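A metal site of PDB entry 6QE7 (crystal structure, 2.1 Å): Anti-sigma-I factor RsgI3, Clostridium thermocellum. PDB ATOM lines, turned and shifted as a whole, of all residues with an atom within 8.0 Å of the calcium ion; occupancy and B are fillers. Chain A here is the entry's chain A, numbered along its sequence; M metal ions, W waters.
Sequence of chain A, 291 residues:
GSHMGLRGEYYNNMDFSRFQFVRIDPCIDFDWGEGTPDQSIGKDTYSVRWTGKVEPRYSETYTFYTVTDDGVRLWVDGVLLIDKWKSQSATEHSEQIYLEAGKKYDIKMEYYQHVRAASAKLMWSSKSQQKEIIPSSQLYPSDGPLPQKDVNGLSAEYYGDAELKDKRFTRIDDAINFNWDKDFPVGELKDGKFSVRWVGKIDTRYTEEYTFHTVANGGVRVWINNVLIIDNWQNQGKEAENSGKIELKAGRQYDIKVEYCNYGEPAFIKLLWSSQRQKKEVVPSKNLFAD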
ATOM      1  N   TYR A  11     -25.202 -33.104 -27.080  1.00  0.00           N
ATOM      2  CA  TYR A  11     -23.778 -32.913 -26.727  1.00  0.00           C
ATOM      3  C   TYR A  11     -23.529 -31.396 -26.741  1.00  0.00           C
ATOM      4  O   TYR A  11     -24.014 -30.766 -27.677  1.00  0.00           O
ATOM      5  CB  TYR A  11     -22.951 -33.631 -27.799  1.00  0.00           C
ATOM      6  CG  TYR A  11     -23.106 -35.124 -27.863  1.00  0.00           C
ATOM      7  CD1 TYR A  11     -24.161 -35.693 -28.576  1.00  0.00           C
ATOM      8  CD2 TYR A  11     -22.143 -35.966 -27.324  1.00  0.00           C
ATOM      9  CE1 TYR A  11     -24.304 -37.058 -28.676  1.00  0.00           C
ATOM     10  CE2 TYR A  11     -22.256 -37.333 -27.405  1.00  0.00           C
ATOM     11  CZ  TYR A  11     -23.337 -37.859 -28.084  1.00  0.00           C
ATOM     12  OH  TYR A  11     -23.478 -39.186 -28.106  1.00  0.00           O
ATOM     13  N   ASN A  12     -22.603 -30.899 -25.916  1.00  0.00           N
ATOM     14  CA  ASN A  12     -22.247 -29.462 -25.803  1.00  0.00           C
ATOM     15  C   ASN A  12     -21.107 -29.045 -26.726  1.00  0.00           C
ATOM     16  O   ASN A  12     -20.755 -27.843 -26.716  1.00  0.00           O
ATOM     17  CB  ASN A  12     -21.869 -29.092 -24.351  1.00  0.00           C
ATOM     18  CG  ASN A  12     -23.047 -28.469 -23.643  1.00  0.00           C
ATOM     19  OD1 ASN A  12     -23.656 -27.580 -24.222  1.00  0.00           O
ATOM     20  ND2 ASN A  12     -23.408 -28.944 -22.452  1.00  0.00           N
ATOM     21  N   ASN A  13     -20.543 -29.987 -27.471  1.00  0.00           N
ATOM     22  CA  ASN A  13     -19.634 -29.727 -28.630  1.00  0.00           C
ATOM     23  C   ASN A  13     -20.396 -30.133 -29.923  1.00  0.00           C
ATOM     24  O   ASN A  13     -21.420 -30.876 -29.834  1.00  0.00           O
ATOM     25  CB  ASN A  13     -18.327 -30.507 -28.450  1.00  0.00           C
ATOM     26  CG  ASN A  13     -17.296 -29.767 -27.611  1.00  0.00           C
ATOM     27  OD1 ASN A  13     -17.403 -28.565 -27.384  1.00  0.00           O
ATOM     28  ND2 ASN A  13     -16.216 -30.449 -27.249  1.00  0.00           N
ATOM     29  N   MET A  14     -19.865 -29.758 -31.092  1.00  0.00           N
ATOM     30  CA  MET A  14     -20.529 -29.967 -32.400  1.00  0.00           C
ATOM     31  C   MET A  14     -20.043 -31.247 -33.056  1.00  0.00           C
ATOM     32  O   MET A  14     -20.514 -31.593 -34.139  1.00  0.00           O
ATOM     33  CB  MET A  14     -20.346 -28.731 -33.287  1.00  0.00           C
ATOM     34  CG  MET A  14     -19.007 -28.507 -33.953  1.00  0.00           C
ATOM     35  SD  MET A  14     -19.356 -26.714 -34.445  1.00  0.00           S
ATOM     36  CE  MET A  14     -17.675 -26.172 -34.827  1.00  0.00           C
ATOM     37  N   SER A  17     -18.962 -34.839 -28.814  1.00  0.00           N
ATOM     38  CA  SER A  17     -18.214 -34.877 -27.540  1.00  0.00           C
ATOM     39  C   SER A  17     -18.890 -33.902 -26.585  1.00  0.00           C
ATOM     40  O   SER A  17     -19.759 -33.026 -27.026  1.00  0.00           O
ATOM     41  CB  SER A  17     -16.731 -34.579 -27.700  1.00  0.00           C
ATOM     42  OG  SER A  17     -16.555 -33.212 -28.121  1.00  0.00           O
ATOM     43  N   ARG A  18     -18.528 -34.035 -25.311  1.00  0.00           N
ATOM     44  CA  ARG A  18     -19.177 -33.338 -24.163  1.00  0.00           C
ATOM     45  C   ARG A  18     -20.651 -33.710 -24.114  1.00  0.00           C
ATOM     46  O   ARG A  18     -21.529 -32.826 -24.131  1.00  0.00           O
ATOM     47  CB  ARG A  18     -18.991 -31.844 -24.311  1.00  0.00           C
ATOM     48  CG  ARG A  18     -17.687 -31.345 -23.731  1.00  0.00           C
ATOM     49  CD  ARG A  18     -17.676 -29.867 -23.937  1.00  0.00           C
ATOM     50  NE  ARG A  18     -16.382 -29.283 -23.706  1.00  0.00           N
ATOM     51  CZ  ARG A  18     -15.896 -28.984 -22.504  1.00  0.00           C
ATOM     52  NH1 ARG A  18     -16.558 -29.288 -21.403  1.00  0.00           N
ATOM     53  NH2 ARG A  18     -14.727 -28.378 -22.415  1.00  0.00           N
ATOM     54  N   ILE A  41     -27.578 -27.193 -22.199  1.00  0.00           N
ATOM     55  CA  ILE A  41     -26.763 -26.996 -23.433  1.00  0.00           C
ATOM     56  C   ILE A  41     -26.404 -25.524 -23.601  1.00  0.00           C
ATOM     57  O   ILE A  41     -27.289 -24.677 -23.912  1.00  0.00           O
ATOM     58  CB  ILE A  41     -27.533 -27.504 -24.669  1.00  0.00           C
ATOM     59  CG1 ILE A  41     -27.801 -29.001 -24.562  1.00  0.00           C
ATOM     60  CG2 ILE A  41     -26.795 -27.125 -25.975  1.00  0.00           C
ATOM     61  CD1 ILE A  41     -26.561 -29.875 -24.313  1.00  0.00           C
ATOM     62  N   GLY A  42     -25.141 -25.236 -23.681  1.00  0.00           N
ATOM     63  CA  GLY A  42     -24.700 -23.845 -23.967  1.00  0.00           C
ATOM     64  C   GLY A  42     -24.968 -23.340 -25.373  1.00  0.00           C
ATOM     65  O   GLY A  42     -24.924 -24.132 -26.339  1.00  0.00           O
ATOM     66  N   LYS A  43     -25.100 -22.017 -25.519  1.00  0.00           N
ATOM     67  CA  LYS A  43     -25.197 -21.312 -26.807  1.00  0.00           C
ATOM     68  C   LYS A  43     -24.036 -21.721 -27.681  1.00  0.00           C
ATOM     69  O   LYS A  43     -22.884 -21.687 -27.224  1.00  0.00           O
ATOM     70  CB  LYS A  43     -25.071 -19.797 -26.717  1.00  0.00           C
ATOM     71  CG  LYS A  43     -25.648 -19.063 -27.923  1.00  0.00           C
ATOM     72  CD  LYS A  43     -25.479 -17.531 -27.775  1.00  0.00           C
ATOM     73  CE  LYS A  43     -25.472 -16.788 -29.080  1.00  0.00           C
ATOM     74  NZ  LYS A  43     -26.782 -16.911 -29.759  1.00  0.00           N
ATOM     75  N   ASP A  44     -24.368 -22.130 -28.894  1.00  0.00           N
ATOM     76  CA  ASP A  44     -23.411 -22.398 -29.984  1.00  0.00           C
ATOM     77  C   ASP A  44     -22.690 -23.752 -29.797  1.00  0.00           C
ATOM     78  O   ASP A  44     -22.645 -24.311 -28.685  1.00  0.00           O
ATOM     79  CB  ASP A  44     -22.431 -21.226 -30.200  1.00  0.00           C
ATOM     80  CG  ASP A  44     -23.047 -19.923 -30.690  1.00  0.00           C
ATOM     81  OD1 ASP A  44     -24.143 -20.006 -31.212  1.00  0.00           O
ATOM     82  OD2 ASP A  44     -22.402 -18.805 -30.536  1.00  0.00           O
ATOM     83  N   THR A  45     -22.149 -24.233 -30.936  1.00  0.00           N
ATOM     84  CA  THR A  45     -21.336 -25.467 -31.089  1.00  0.00           C
ATOM     85  C   THR A  45     -21.974 -26.596 -30.283  1.00  0.00           C
ATOM     86  O   THR A  45     -21.380 -27.011 -29.288  1.00  0.00           O
ATOM     87  CB  THR A  45     -19.896 -25.188 -30.633  1.00  0.00           C
ATOM     88  OG1 THR A  45     -20.016 -24.681 -29.311  1.00  0.00           O
ATOM     89  CG2 THR A  45     -19.151 -24.177 -31.465  1.00  0.00           C
ATOM     90  N   TYR A  46     -23.112 -27.124 -30.723  1.00  0.00           N
ATOM     91  CA  TYR A  46     -23.726 -28.281 -30.089  1.00  0.00           C
ATOM     92  C   TYR A  46     -24.132 -29.253 -31.193  1.00  0.00           C
ATOM     93  O   TYR A  46     -24.094 -28.843 -32.393  1.00  0.00           O
ATOM     94  CB  TYR A  46     -24.847 -27.905 -29.105  1.00  0.00           C
ATOM     95  CG  TYR A  46     -25.980 -27.061 -29.611  1.00  0.00           C
ATOM     96  CD1 TYR A  46     -27.070 -27.631 -30.207  1.00  0.00           C
ATOM     97  CD2 TYR A  46     -26.041 -25.679 -29.366  1.00  0.00           C
ATOM     98  CE1 TYR A  46     -28.170 -26.881 -30.626  1.00  0.00           C
ATOM     99  CE2 TYR A  46     -27.176 -24.931 -29.668  1.00  0.00           C
ATOM    100  CZ  TYR A  46     -28.223 -25.523 -30.359  1.00  0.00           C
ATOM    101  OH  TYR A  46     -29.335 -24.815 -30.741  1.00  0.00           O
ATOM    102  N   SER A  47     -24.395 -30.484 -30.762  1.00  0.00           N
ATOM    103  CA  SER A  47     -24.750 -31.589 -31.671  1.00  0.00           C
ATOM    104  C   SER A  47     -25.721 -32.534 -30.992  1.00  0.00           C
ATOM    105  O   SER A  47     -25.732 -32.602 -29.764  1.00  0.00           O
ATOM    106  CB  SER A  47     -23.554 -32.307 -32.261  1.00  0.00           C
ATOM    107  OG  SER A  47     -22.653 -32.827 -31.273  1.00  0.00           O
ATOM    108  N   GLN A 113     -25.282 -27.509 -34.735  1.00  0.00           N
ATOM    109  CA  GLN A 113     -25.293 -26.038 -34.712  1.00  0.00           C
ATOM    110  C   GLN A 113     -23.874 -25.517 -34.541  1.00  0.00           C
ATOM    111  O   GLN A 113     -23.097 -25.979 -33.618  1.00  0.00           O
ATOM    112  CB  GLN A 113     -26.191 -25.584 -33.546  1.00  0.00           C
ATOM    113  CG  GLN A 113     -25.789 -24.216 -32.975  1.00  0.00           C
ATOM    114  CD  GLN A 113     -26.157 -23.031 -33.813  1.00  0.00           C
ATOM    115  OE1 GLN A 113     -26.133 -23.065 -35.031  1.00  0.00           O
ATOM    116  NE2 GLN A 113     -26.648 -21.980 -33.135  1.00  0.00           N
ATOM    117  N   HIS A 114     -23.548 -24.547 -35.380  1.00  0.00           N
ATOM    118  CA  HIS A 114     -22.295 -23.770 -35.236  1.00  0.00           C
ATOM    119  C   HIS A 114     -22.619 -22.499 -34.454  1.00  0.00           C
ATOM    120  O   HIS A 114     -22.409 -22.519 -33.230  1.00  0.00           O
ATOM    121  CB  HIS A 114     -21.591 -23.546 -36.593  1.00  0.00           C
ATOM    122  CG  HIS A 114     -20.271 -22.862 -36.442  1.00  0.00           C
ATOM    123  ND1 HIS A 114     -19.894 -21.858 -37.282  1.00  0.00           N
ATOM    124  CD2 HIS A 114     -19.303 -22.945 -35.469  1.00  0.00           C
ATOM    125  CE1 HIS A 114     -18.723 -21.344 -36.879  1.00  0.00           C
ATOM    126  NE2 HIS A 114     -18.337 -22.017 -35.761  1.00  0.00           N
ATOM    127  N   ASP A 203     -10.208 -29.382 -26.122  1.00  0.00           N
ATOM    128  CA  ASP A 203     -11.028 -28.394 -26.860  1.00  0.00           C
ATOM    129  C   ASP A 203     -10.760 -27.030 -26.265  1.00  0.00           C
ATOM    130  O   ASP A 203     -10.118 -26.903 -25.190  1.00  0.00           O
ATOM    131  CB  ASP A 203     -12.521 -28.716 -26.938  1.00  0.00           C
ATOM    132  CG  ASP A 203     -13.231 -28.838 -25.606  1.00  0.00           C
ATOM    133  OD1 ASP A 203     -12.687 -28.343 -24.594  1.00  0.00           O
ATOM    134  OD2 ASP A 203     -14.240 -29.592 -25.568  1.00  0.00           O
ATOM    135  N   ALA A 250     -13.052 -23.649 -31.856  1.00  0.00           N
ATOM    136  CA  ALA A 250     -13.881 -23.926 -30.663  1.00  0.00           C
ATOM    137  C   ALA A 250     -14.958 -24.923 -31.038  1.00  0.00           C
ATOM    138  O   ALA A 250     -15.421 -24.945 -32.191  1.00  0.00           O
ATOM    139  CB  ALA A 250     -14.474 -22.640 -30.154  1.00  0.00           C
ATOM    140  N   GLY A 251     -15.372 -25.696 -30.074  1.00  0.00           N
ATOM    141  CA  GLY A 251     -16.579 -26.509 -30.174  1.00  0.00           C
ATOM    142  C   GLY A 251     -16.270 -27.913 -30.627  1.00  0.00           C
ATOM    143  O   GLY A 251     -17.219 -28.579 -30.975  1.00  0.00           O
ATOM    144  N   ARG A 252     -15.012 -28.314 -30.766  1.00  0.00           N
ATOM    145  CA  ARG A 252     -14.667 -29.702 -31.145  1.00  0.00           C
ATOM    146  C   ARG A 252     -13.393 -30.159 -30.423  1.00  0.00           C
ATOM    147  O   ARG A 252     -12.661 -29.323 -30.075  1.00  0.00           O
ATOM    148  CB  ARG A 252     -14.532 -29.860 -32.665  1.00  0.00           C
ATOM    149  CG  ARG A 252     -13.616 -28.866 -33.354  1.00  0.00           C
ATOM    150  CD  ARG A 252     -13.028 -29.422 -34.638  1.00  0.00           C
ATOM    151  NE  ARG A 252     -12.160 -30.591 -34.401  1.00  0.00           N
ATOM    152  CZ  ARG A 252     -11.508 -31.298 -35.359  1.00  0.00           C
ATOM    153  NH1 ARG A 252     -11.587 -30.977 -36.644  1.00  0.00           N
ATOM    154  NH2 ARG A 252     -10.792 -32.348 -35.008  1.00  0.00           N
HETATM  155 CA    CA M   1     -20.908 -25.657 -27.314  1.00  0.00          CA
HETATM  156  O   HOH W   1     -18.535 -26.064 -26.956  1.00  0.00           O
HETATM  157  O   HOH W   2     -21.010 -23.279 -26.738  1.00  0.00           O
HETATM  158  O   HOH W   3     -23.179 -25.975 -26.445  1.00  0.00           O
HETATM  159  O   HOH W   4     -20.445 -25.512 -24.893  1.00  0.00           O
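Water W3 bridges O of Gly 42 and OD1 of Asn 12.
Within 4 Å of the calcium ion: Asn 12, Asp 44 and Thr 45.
The nearest printed residue that does not touch the calcium ion is Tyr 46 (4.3 Å).
O of Asn 12 binds the calcium ion (2.3 Å).
OG1 of Thr 45 binds the calcium ion, at 2.4 Å.
The calcium ion is bound by water W1 (2.4 Å).
The calcium ion is bound by O of Thr 45, 2.4 Å away.
Water W2 binds the calcium ion, at 2.4 Å.
Water W3 binds the calcium ion (2.5 Å).
The calcium ion is bound by water W4 (2.5 Å).
The calcium ion is bound by O of Asp 44, 2.6 Å away.
N of Gly 42 sits at hydrogen-bond distance from OD1 of Asn 12, 2.8 Å away.
The backbone carbonyl oxygen of Arg 18 lies within hydrogen-bond range of the backbone NH of Asn 12 (2.8 Å).
N of Thr 45 lies close to O of Gln 113 (3.3 Å).
O of His 114 is in hydrogen-bond range of N of Thr 45 (2.9 Å).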
